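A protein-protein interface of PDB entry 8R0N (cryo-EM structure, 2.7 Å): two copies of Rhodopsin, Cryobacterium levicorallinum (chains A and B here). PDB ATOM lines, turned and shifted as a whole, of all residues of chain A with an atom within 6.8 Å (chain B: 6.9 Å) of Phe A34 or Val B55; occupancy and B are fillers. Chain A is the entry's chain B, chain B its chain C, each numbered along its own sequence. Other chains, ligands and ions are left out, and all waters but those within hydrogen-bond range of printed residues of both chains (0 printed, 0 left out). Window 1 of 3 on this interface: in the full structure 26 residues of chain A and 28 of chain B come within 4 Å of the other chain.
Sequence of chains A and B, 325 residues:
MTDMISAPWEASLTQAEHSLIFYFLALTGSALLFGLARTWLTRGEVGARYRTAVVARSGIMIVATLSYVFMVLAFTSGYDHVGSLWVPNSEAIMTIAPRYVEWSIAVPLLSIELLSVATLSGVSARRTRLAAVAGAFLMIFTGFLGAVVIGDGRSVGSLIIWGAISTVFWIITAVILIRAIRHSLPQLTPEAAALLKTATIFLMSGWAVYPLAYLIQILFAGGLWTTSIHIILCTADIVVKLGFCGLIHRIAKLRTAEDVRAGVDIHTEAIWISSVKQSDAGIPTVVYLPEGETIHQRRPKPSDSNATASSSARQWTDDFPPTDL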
ATOM      1  N   GLY A  29      37.760 -15.993   5.797  1.00  0.00           N
ATOM      2  CA  GLY A  29      36.706 -15.049   6.102  1.00  0.00           C
ATOM      3  C   GLY A  29      35.380 -15.742   6.399  1.00  0.00           C
ATOM      4  O   GLY A  29      34.606 -15.269   7.227  1.00  0.00           O
ATOM      5  N   SER A  30      35.115 -16.842   5.690  1.00  0.00           N
ATOM      6  CA  SER A  30      33.880 -17.578   5.870  1.00  0.00           C
ATOM      7  C   SER A  30      33.891 -18.251   7.231  1.00  0.00           C
ATOM      8  O   SER A  30      32.912 -18.168   7.962  1.00  0.00           O
ATOM      9  CB  SER A  30      33.696 -18.599   4.780  1.00  0.00           C
ATOM     10  OG  SER A  30      33.682 -17.961   3.519  1.00  0.00           O
ATOM     11  N   ALA A  31      35.004 -18.903   7.556  1.00  0.00           N
ATOM     12  CA  ALA A  31      35.087 -19.610   8.812  1.00  0.00           C
ATOM     13  C   ALA A  31      34.902 -18.636   9.978  1.00  0.00           C
ATOM     14  O   ALA A  31      34.303 -18.995  10.981  1.00  0.00           O
ATOM     15  CB  ALA A  31      36.369 -20.365   8.886  1.00  0.00           C
ATOM     16  N   LEU A  32      35.383 -17.406   9.844  1.00  0.00           N
ATOM     17  CA  LEU A  32      35.306 -16.466  10.938  1.00  0.00           C
ATOM     18  C   LEU A  32      33.890 -15.947  11.055  1.00  0.00           C
ATOM     19  O   LEU A  32      33.454 -15.604  12.149  1.00  0.00           O
ATOM     20  CB  LEU A  32      36.304 -15.329  10.727  1.00  0.00           C
ATOM     21  CG  LEU A  32      37.757 -15.792  10.761  1.00  0.00           C
ATOM     22  CD1 LEU A  32      38.682 -14.650  10.404  1.00  0.00           C
ATOM     23  CD2 LEU A  32      38.121 -16.356  12.113  1.00  0.00           C
ATOM     24  N   LEU A  33      33.160 -15.939   9.956  1.00  0.00           N
ATOM     25  CA  LEU A  33      31.776 -15.535  10.036  1.00  0.00           C
ATOM     26  C   LEU A  33      30.933 -16.645  10.677  1.00  0.00           C
ATOM     27  O   LEU A  33      29.965 -16.366  11.382  1.00  0.00           O
ATOM     28  CB  LEU A  33      31.293 -15.177   8.633  1.00  0.00           C
ATOM     29  CG  LEU A  33      29.963 -14.440   8.608  1.00  0.00           C
ATOM     30  CD1 LEU A  33      29.930 -13.261   9.581  1.00  0.00           C
ATOM     31  CD2 LEU A  33      29.696 -13.950   7.213  1.00  0.00           C
ATOM     32  N   PHE A  34      31.317 -17.894  10.452  1.00  0.00           N
ATOM     33  CA  PHE A  34      30.696 -18.990  11.154  1.00  0.00           C
ATOM     34  C   PHE A  34      30.959 -18.829  12.654  1.00  0.00           C
ATOM     35  O   PHE A  34      30.041 -18.911  13.473  1.00  0.00           O
ATOM     36  CB  PHE A  34      31.214 -20.319  10.613  1.00  0.00           C
ATOM     37  CG  PHE A  34      31.003 -21.464  11.553  1.00  0.00           C
ATOM     38  CD1 PHE A  34      29.729 -21.869  11.926  1.00  0.00           C
ATOM     39  CD2 PHE A  34      32.084 -22.117  12.101  1.00  0.00           C
ATOM     40  CE1 PHE A  34      29.555 -22.942  12.790  1.00  0.00           C
ATOM     41  CE2 PHE A  34      31.913 -23.157  13.007  1.00  0.00           C
ATOM     42  CZ  PHE A  34      30.655 -23.570  13.358  1.00  0.00           C
ATOM     43  N   GLY A  35      32.224 -18.589  13.004  1.00  0.00           N
ATOM     44  CA  GLY A  35      32.618 -18.389  14.378  1.00  0.00           C
ATOM     45  C   GLY A  35      31.830 -17.262  15.044  1.00  0.00           C
ATOM     46  O   GLY A  35      31.525 -17.331  16.229  1.00  0.00           O
ATOM     47  N   LEU A  36      31.538 -16.211  14.309  1.00  0.00           N
ATOM     48  CA  LEU A  36      30.808 -15.116  14.897  1.00  0.00           C
ATOM     49  C   LEU A  36      29.393 -15.572  15.235  1.00  0.00           C
ATOM     50  O   LEU A  36      28.907 -15.331  16.333  1.00  0.00           O
ATOM     51  CB  LEU A  36      30.784 -13.963  13.903  1.00  0.00           C
ATOM     52  CG  LEU A  36      30.090 -12.693  14.379  1.00  0.00           C
ATOM     53  CD1 LEU A  36      30.632 -12.192  15.721  1.00  0.00           C
ATOM     54  CD2 LEU A  36      30.272 -11.617  13.341  1.00  0.00           C
ATOM     55  N   ALA A  37      28.761 -16.276  14.305  1.00  0.00           N
ATOM     56  CA  ALA A  37      27.447 -16.812  14.551  1.00  0.00           C
ATOM     57  C   ALA A  37      27.476 -17.742  15.757  1.00  0.00           C
ATOM     58  O   ALA A  37      26.608 -17.636  16.608  1.00  0.00           O
ATOM     59  CB  ALA A  37      26.967 -17.528  13.312  1.00  0.00           C
ATOM     60  N   ARG A  38      28.451 -18.647  15.811  1.00  0.00           N
ATOM     61  CA  ARG A  38      28.540 -19.611  16.883  1.00  0.00           C
ATOM     62  C   ARG A  38      28.631 -18.886  18.229  1.00  0.00           C
ATOM     63  O   ARG A  38      28.102 -19.355  19.236  1.00  0.00           O
ATOM     64  CB  ARG A  38      29.746 -20.523  16.640  1.00  0.00           C
ATOM     65  CG  ARG A  38      30.030 -21.442  17.816  1.00  0.00           C
ATOM     66  CD  ARG A  38      30.821 -22.645  17.432  1.00  0.00           C
ATOM     67  NE  ARG A  38      32.189 -22.294  17.139  1.00  0.00           N
ATOM     68  CZ  ARG A  38      33.261 -22.949  17.577  1.00  0.00           C
ATOM     69  NH1 ARG A  38      34.462 -22.433  17.396  1.00  0.00           N
ATOM     70  NH2 ARG A  38      33.140 -24.090  18.237  1.00  0.00           N
ATOM     71  N   THR A  39      29.322 -17.750  18.237  1.00  0.00           N
ATOM     72  CA  THR A  39      29.570 -17.027  19.461  1.00  0.00           C
ATOM     73  C   THR A  39      28.266 -16.448  19.970  1.00  0.00           C
ATOM     74  O   THR A  39      27.980 -16.543  21.152  1.00  0.00           O
ATOM     75  CB  THR A  39      30.677 -15.983  19.272  1.00  0.00           C
ATOM     76  OG1 THR A  39      31.870 -16.720  18.967  1.00  0.00           O
ATOM     77  CG2 THR A  39      30.935 -15.166  20.521  1.00  0.00           C
ATOM     78  N   LEU A  41      25.268 -17.510  19.154  1.00  0.00           N
ATOM     79  CA  LEU A  41      24.253 -18.513  19.360  1.00  0.00           C
ATOM     80  C   LEU A  41      24.503 -19.253  20.656  1.00  0.00           C
ATOM     81  O   LEU A  41      23.609 -19.920  21.145  1.00  0.00           O
ATOM     82  CB  LEU A  41      24.239 -19.476  18.181  1.00  0.00           C
ATOM     83  CG  LEU A  41      23.673 -18.910  16.884  1.00  0.00           C
ATOM     84  CD1 LEU A  41      23.923 -19.882  15.755  1.00  0.00           C
ATOM     85  CD2 LEU A  41      22.191 -18.646  16.980  1.00  0.00           C
ATOM     86  N   THR A  42      25.693 -19.149  21.215  1.00  0.00           N
ATOM     87  CA  THR A  42      26.021 -19.966  22.370  1.00  0.00           C
ATOM     88  C   THR A  42      26.370 -19.064  23.535  1.00  0.00           C
ATOM     89  O   THR A  42      26.833 -19.569  24.543  1.00  0.00           O
ATOM     90  CB  THR A  42      27.158 -20.942  22.041  1.00  0.00           C
ATOM     91  OG1 THR A  42      28.341 -20.218  21.665  1.00  0.00           O
ATOM     92  CG2 THR A  42      26.763 -21.903  20.939  1.00  0.00           C
ATOM     93  N   GLU A  45      25.224 -19.893  27.282  1.00  0.00           N
ATOM     94  CA  GLU A  45      25.600 -21.151  27.891  1.00  0.00           C
ATOM     95  C   GLU A  45      26.511 -20.864  29.070  1.00  0.00           C
ATOM     96  O   GLU A  45      26.794 -21.742  29.883  1.00  0.00           O
ATOM     97  CB  GLU A  45      26.282 -22.026  26.852  1.00  0.00           C
ATOM     98  CG  GLU A  45      25.392 -22.309  25.667  1.00  0.00           C
ATOM     99  CD  GLU A  45      25.948 -23.214  24.579  1.00  0.00           C
ATOM    100  OE1 GLU A  45      25.144 -23.585  23.693  1.00  0.00           O
ATOM    101  OE2 GLU A  45      27.170 -23.577  24.610  1.00  0.00           O
ATOM    102  N   MET A  61      35.996 -12.164  16.559  1.00  0.00           N
ATOM    103  CA  MET A  61      35.379 -12.699  15.367  1.00  0.00           C
ATOM    104  C   MET A  61      34.951 -11.548  14.479  1.00  0.00           C
ATOM    105  O   MET A  61      35.035 -11.671  13.267  1.00  0.00           O
ATOM    106  CB  MET A  61      34.144 -13.544  15.669  1.00  0.00           C
ATOM    107  CG  MET A  61      34.409 -14.810  16.434  1.00  0.00           C
ATOM    108  SD  MET A  61      35.577 -15.944  15.663  1.00  0.00           S
ATOM    109  CE  MET A  61      36.897 -15.734  16.849  1.00  0.00           C
ATOM    110  N   THR A  65      36.642 -10.827  10.841  1.00  0.00           N
ATOM    111  CA  THR A  65      35.792 -11.057   9.691  1.00  0.00           C
ATOM    112  C   THR A  65      35.868  -9.853   8.764  1.00  0.00           C
ATOM    113  O   THR A  65      35.924 -10.046   7.549  1.00  0.00           O
ATOM    114  CB  THR A  65      34.338 -11.331  10.084  1.00  0.00           C
ATOM    115  OG1 THR A  65      34.322 -12.420  11.002  1.00  0.00           O
ATOM    116  CG2 THR A  65      33.481 -11.697   8.895  1.00  0.00           C
ATOM    117  N   LEU A 242      39.204 -20.404  15.801  1.00  0.00           N
ATOM    118  CA  LEU A 242      38.096 -21.339  15.981  1.00  0.00           C
ATOM    119  C   LEU A 242      38.407 -22.331  17.085  1.00  0.00           C
ATOM    120  O   LEU A 242      37.579 -22.551  17.958  1.00  0.00           O
ATOM    121  CB  LEU A 242      37.798 -22.084  14.688  1.00  0.00           C
ATOM    122  CG  LEU A 242      37.105 -21.241  13.621  1.00  0.00           C
ATOM    123  CD1 LEU A 242      36.597 -22.118  12.495  1.00  0.00           C
ATOM    124  CD2 LEU A 242      35.945 -20.449  14.191  1.00  0.00           C
ATOM    125  N   THR B  39      16.385 -20.455  10.516  1.00  0.00           N
ATOM    126  CA  THR B  39      17.261 -21.080  11.477  1.00  0.00           C
ATOM    127  C   THR B  39      17.265 -20.262  12.752  1.00  0.00           C
ATOM    128  O   THR B  39      17.174 -20.819  13.833  1.00  0.00           O
ATOM    129  CB  THR B  39      18.658 -21.311  10.889  1.00  0.00           C
ATOM    130  OG1 THR B  39      18.484 -22.239   9.810  1.00  0.00           O
ATOM    131  CG2 THR B  39      19.628 -21.919  11.884  1.00  0.00           C
ATOM    132  N   TYR B  50      21.244 -30.156  22.003  1.00  0.00           N
ATOM    133  CA  TYR B  50      21.296 -30.313  20.559  1.00  0.00           C
ATOM    134  C   TYR B  50      21.580 -28.984  19.883  1.00  0.00           C
ATOM    135  O   TYR B  50      21.414 -28.889  18.673  1.00  0.00           O
ATOM    136  CB  TYR B  50      20.032 -30.980  20.011  1.00  0.00           C
ATOM    137  CG  TYR B  50      19.676 -32.230  20.781  1.00  0.00           C
ATOM    138  CD1 TYR B  50      20.384 -33.415  20.684  1.00  0.00           C
ATOM    139  CD2 TYR B  50      18.657 -32.177  21.692  1.00  0.00           C
ATOM    140  CE1 TYR B  50      20.055 -34.537  21.431  1.00  0.00           C
ATOM    141  CE2 TYR B  50      18.308 -33.287  22.447  1.00  0.00           C
ATOM    142  CZ  TYR B  50      19.031 -34.456  22.348  1.00  0.00           C
ATOM    143  OH  TYR B  50      18.676 -35.487  23.174  1.00  0.00           O
ATOM    144  N   ARG B  51      22.127 -28.005  20.602  1.00  0.00           N
ATOM    145  CA  ARG B  51      22.335 -26.687  20.023  1.00  0.00           C
ATOM    146  C   ARG B  51      23.399 -26.701  18.923  1.00  0.00           C
ATOM    147  O   ARG B  51      23.495 -25.757  18.153  1.00  0.00           O
ATOM    148  CB  ARG B  51      22.715 -25.708  21.125  1.00  0.00           C
ATOM    149  CG  ARG B  51      22.862 -24.256  20.677  1.00  0.00           C
ATOM    150  CD  ARG B  51      22.764 -23.242  21.809  1.00  0.00           C
ATOM    151  NE  ARG B  51      21.556 -23.521  22.583  1.00  0.00           N
ATOM    152  CZ  ARG B  51      21.407 -23.303  23.870  1.00  0.00           C
ATOM    153  NH1 ARG B  51      22.416 -22.856  24.584  1.00  0.00           N
ATOM    154  NH2 ARG B  51      20.241 -23.541  24.437  1.00  0.00           N
ATOM    155  N   THR B  52      24.207 -27.758  18.836  1.00  0.00           N
ATOM    156  CA  THR B  52      25.228 -27.849  17.809  1.00  0.00           C
ATOM    157  C   THR B  52      24.586 -27.905  16.433  1.00  0.00           C
ATOM    158  O   THR B  52      25.113 -27.334  15.479  1.00  0.00           O
ATOM    159  CB  THR B  52      26.103 -29.070  18.040  1.00  0.00           C
ATOM    160  OG1 THR B  52      26.442 -28.994  19.427  1.00  0.00           O
ATOM    161  CG2 THR B  52      27.327 -29.095  17.157  1.00  0.00           C
ATOM    162  N   ALA B  53      23.414 -28.526  16.354  1.00  0.00           N
ATOM    163  CA  ALA B  53      22.692 -28.588  15.103  1.00  0.00           C
ATOM    164  C   ALA B  53      22.339 -27.191  14.601  1.00  0.00           C
ATOM    165  O   ALA B  53      22.447 -26.921  13.414  1.00  0.00           O
ATOM    166  CB  ALA B  53      21.481 -29.447  15.277  1.00  0.00           C
ATOM    167  N   VAL B  54      21.923 -26.311  15.489  1.00  0.00           N
ATOM    168  CA  VAL B  54      21.570 -24.957  15.110  1.00  0.00           C
ATOM    169  C   VAL B  54      22.817 -24.191  14.685  1.00  0.00           C
ATOM    170  O   VAL B  54      22.764 -23.316  13.820  1.00  0.00           O
ATOM    171  CB  VAL B  54      20.911 -24.245  16.302  1.00  0.00           C
ATOM    172  CG1 VAL B  54      20.539 -22.812  15.971  1.00  0.00           C
ATOM    173  CG2 VAL B  54      19.716 -25.030  16.785  1.00  0.00           C
ATOM    174  N   VAL B  55      23.921 -24.476  15.368  1.00  0.00           N
ATOM    175  CA  VAL B  55      25.149 -23.763  15.121  1.00  0.00           C
ATOM    176  C   VAL B  55      25.641 -24.164  13.741  1.00  0.00           C
ATOM    177  O   VAL B  55      25.992 -23.298  12.945  1.00  0.00           O
ATOM    178  CB  VAL B  55      26.171 -24.039  16.234  1.00  0.00           C
ATOM    179  CG1 VAL B  55      27.577 -23.590  15.869  1.00  0.00           C
ATOM    180  CG2 VAL B  55      25.725 -23.354  17.515  1.00  0.00           C
ATOM    181  N   ALA B  56      25.646 -25.461  13.457  1.00  0.00           N
ATOM    182  CA  ALA B  56      26.098 -25.921  12.163  1.00  0.00           C
ATOM    183  C   ALA B  56      25.225 -25.324  11.064  1.00  0.00           C
ATOM    184  O   ALA B  56      25.722 -24.678  10.141  1.00  0.00           O
ATOM    185  CB  ALA B  56      26.096 -27.417  12.126  1.00  0.00           C
ATOM    186  N   ARG B  57      23.919 -25.509  11.193  1.00  0.00           N
ATOM    187  CA  ARG B  57      22.971 -25.023  10.208  1.00  0.00           C
ATOM    188  C   ARG B  57      23.101 -23.516   9.992  1.00  0.00           C
ATOM    189  O   ARG B  57      23.057 -23.038   8.875  1.00  0.00           O
ATOM    190  CB  ARG B  57      21.573 -25.410  10.658  1.00  0.00           C
ATOM    191  CG  ARG B  57      20.514 -25.122   9.621  1.00  0.00           C
ATOM    192  CD  ARG B  57      19.143 -25.484  10.159  1.00  0.00           C
ATOM    193  NE  ARG B  57      19.152 -26.732  10.908  1.00  0.00           N
ATOM    194  CZ  ARG B  57      18.850 -26.837  12.197  1.00  0.00           C
ATOM    195  NH1 ARG B  57      18.967 -28.017  12.779  1.00  0.00           N
ATOM    196  NH2 ARG B  57      18.497 -25.773  12.897  1.00  0.00           N
ATOM    197  N   SER B  58      23.318 -22.758  11.046  1.00  0.00           N
ATOM    198  CA  SER B  58      23.515 -21.326  10.899  1.00  0.00           C
ATOM    199  C   SER B  58      24.750 -21.004  10.076  1.00  0.00           C
ATOM    200  O   SER B  58      24.740 -20.052   9.309  1.00  0.00           O
ATOM    201  CB  SER B  58      23.617 -20.664  12.232  1.00  0.00           C
ATOM    202  OG  SER B  58      22.409 -20.854  12.966  1.00  0.00           O
ATOM    203  N   GLY B  59      25.811 -21.776  10.266  1.00  0.00           N
ATOM    204  CA  GLY B  59      27.047 -21.542   9.550  1.00  0.00           C
ATOM    205  C   GLY B  59      26.877 -21.871   8.082  1.00  0.00           C
ATOM    206  O   GLY B  59      27.191 -21.052   7.216  1.00  0.00           O
ATOM    207  N   ILE B  60      26.293 -23.038   7.825  1.00  0.00           N
ATOM    208  CA  ILE B  60      25.952 -23.414   6.469  1.00  0.00           C
ATOM    209  C   ILE B  60      25.190 -22.293   5.775  1.00  0.00           C
ATOM    210  O   ILE B  60      25.584 -21.859   4.701  1.00  0.00           O
ATOM    211  CB  ILE B  60      25.160 -24.718   6.468  1.00  0.00           C
ATOM    212  CG1 ILE B  60      26.030 -25.855   7.016  1.00  0.00           C
ATOM    213  CG2 ILE B  60      24.676 -25.013   5.076  1.00  0.00           C
ATOM    214  CD1 ILE B  60      25.251 -27.073   7.491  1.00  0.00           C
ATOM    215  N   ILE B  62      24.850 -19.154   6.428  1.00  0.00           N
ATOM    216  CA  ILE B  62      25.526 -17.874   6.278  1.00  0.00           C
ATOM    217  C   ILE B  62      26.543 -17.966   5.150  1.00  0.00           C
ATOM    218  O   ILE B  62      26.545 -17.133   4.250  1.00  0.00           O
ATOM    219  CB  ILE B  62      26.206 -17.416   7.577  1.00  0.00           C
ATOM    220  CG1 ILE B  62      25.196 -17.119   8.668  1.00  0.00           C
ATOM    221  CG2 ILE B  62      27.040 -16.180   7.348  1.00  0.00           C
ATOM    222  CD1 ILE B  62      25.869 -16.782   9.963  1.00  0.00           C
ATOM    223  N   VAL B  63      27.407 -18.965   5.204  1.00  0.00           N
ATOM    224  CA  VAL B  63      28.461 -19.029   4.221  1.00  0.00           C
ATOM    225  C   VAL B  63      27.849 -19.188   2.841  1.00  0.00           C
ATOM    226  O   VAL B  63      28.277 -18.521   1.907  1.00  0.00           O
ATOM    227  CB  VAL B  63      29.500 -20.112   4.524  1.00  0.00           C
ATOM    228  CG1 VAL B  63      30.107 -19.902   5.905  1.00  0.00           C
ATOM    229  CG2 VAL B  63      28.939 -21.501   4.378  1.00  0.00           C
ATOM    230  N   ILE B 105      33.409 -25.258   3.829  1.00  0.00           N
ATOM    231  CA  ILE B 105      32.862 -25.031   5.151  1.00  0.00           C
ATOM    232  C   ILE B 105      31.651 -25.938   5.358  1.00  0.00           C
ATOM    233  O   ILE B 105      31.564 -26.610   6.378  1.00  0.00           O
ATOM    234  CB  ILE B 105      32.498 -23.556   5.335  1.00  0.00           C
ATOM    235  CG1 ILE B 105      33.645 -22.618   4.960  1.00  0.00           C
ATOM    236  CG2 ILE B 105      32.065 -23.311   6.767  1.00  0.00           C
ATOM    237  CD1 ILE B 105      34.789 -22.643   5.931  1.00  0.00           C
ATOM    238  N   LEU B 109      30.470 -28.955   8.049  1.00  0.00           N
ATOM    239  CA  LEU B 109      29.381 -28.566   8.926  1.00  0.00           C
ATOM    240  C   LEU B 109      28.165 -29.480   8.784  1.00  0.00           C
ATOM    241  O   LEU B 109      27.555 -29.794   9.792  1.00  0.00           O
ATOM    242  CB  LEU B 109      29.008 -27.107   8.718  1.00  0.00           C
ATOM    243  CG  LEU B 109      29.951 -26.107   9.383  1.00  0.00           C
ATOM    244  CD1 LEU B 109      29.452 -24.686   9.185  1.00  0.00           C
ATOM    245  CD2 LEU B 109      30.149 -26.354  10.887  1.00  0.00           C
ATOM    246  N   ILE B 112      28.704 -32.440  10.814  1.00  0.00           N
ATOM    247  CA  ILE B 112      28.579 -32.162  12.224  1.00  0.00           C
ATOM    248  C   ILE B 112      27.115 -32.105  12.599  1.00  0.00           C
ATOM    249  O   ILE B 112      26.748 -32.694  13.614  1.00  0.00           O
ATOM    250  CB  ILE B 112      29.330 -30.875  12.590  1.00  0.00           C
ATOM    251  CG1 ILE B 112      30.833 -31.157  12.530  1.00  0.00           C
ATOM    252  CG2 ILE B 112      28.909 -30.346  13.951  1.00  0.00           C
ATOM    253  CD1 ILE B 112      31.650 -29.979  12.863  1.00  0.00           C
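OE1 of Glu A45 is in salt-bridge range of NH1 of Arg B51 (3.0 Å).
OG of Ser B58 is in hydrogen-bond range of O of Val B54 (2.6 Å).
The backbone carbonyl oxygen (O) of Arg A38 sits at hydrogen-bond distance from the side-chain hydroxyl (OG1) of Thr A42 (2.6 Å).
NH1 of Arg A38 sits at hydrogen-bond distance from O of Leu A242, 3.2 Å away.
Ser A30 touches Val B63 (O to CG1, 3.9 Å).
CD2 of Leu A33 touches CG2 of Ile B62 (3.5 Å).
Val B55 touches Phe A34 (O to CE1, 3.6 Å).
Phe A34 touches Gly B59 (CD1 to CA, 3.6 Å).
CD2 of Leu B109 touches CZ of Phe A34, at 3.8 Å.
CD1 of Ile B62 touches CB of Ala A37, 3.6 Å away.
Val B55 touches Arg A38.
Leu A41 touches Arg B51 (O to CD, 3.5 Å).
Leu A41 touches Ser B58.
CG2 of Val B55 touches CG2 of Thr A42, at 3.9 Å.
Of the printed residues of chain B, Leu A33 touches Ile B62.
Of the printed residues of chain B, Ala A37 touches Ile B62.
Printed residues of chain B within 4 Å of Arg A38: Val B55.
Of the printed residues of chain B, Thr A42 touches Val B55.
The nearest residue of chain B that does not touch Phe A34 is Ala B56 (4.6 Å).
Of the 17 printed residues of chain A, 8 touch a printed residue of chain B.
Printed residues of chain A that touch a printed residue of chain B: Ser A30, Leu A33, Phe A34, Ala A37, Arg A38, Leu A41, Thr A42 and Glu A45.
Hydrophobic or aromatic side chains of chain A that line the printed part of chain B: Leu A33, Phe A34, Ala A37 and Leu A41.
Hydrophobic or aromatic side chains of chain B within 4 Å of the printed part of chain A: Val B55, Ile B62, Val B63 and Leu B109.
Among the printed residues, 11 pairs touch across the chains.
1 position is printed for both chains.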
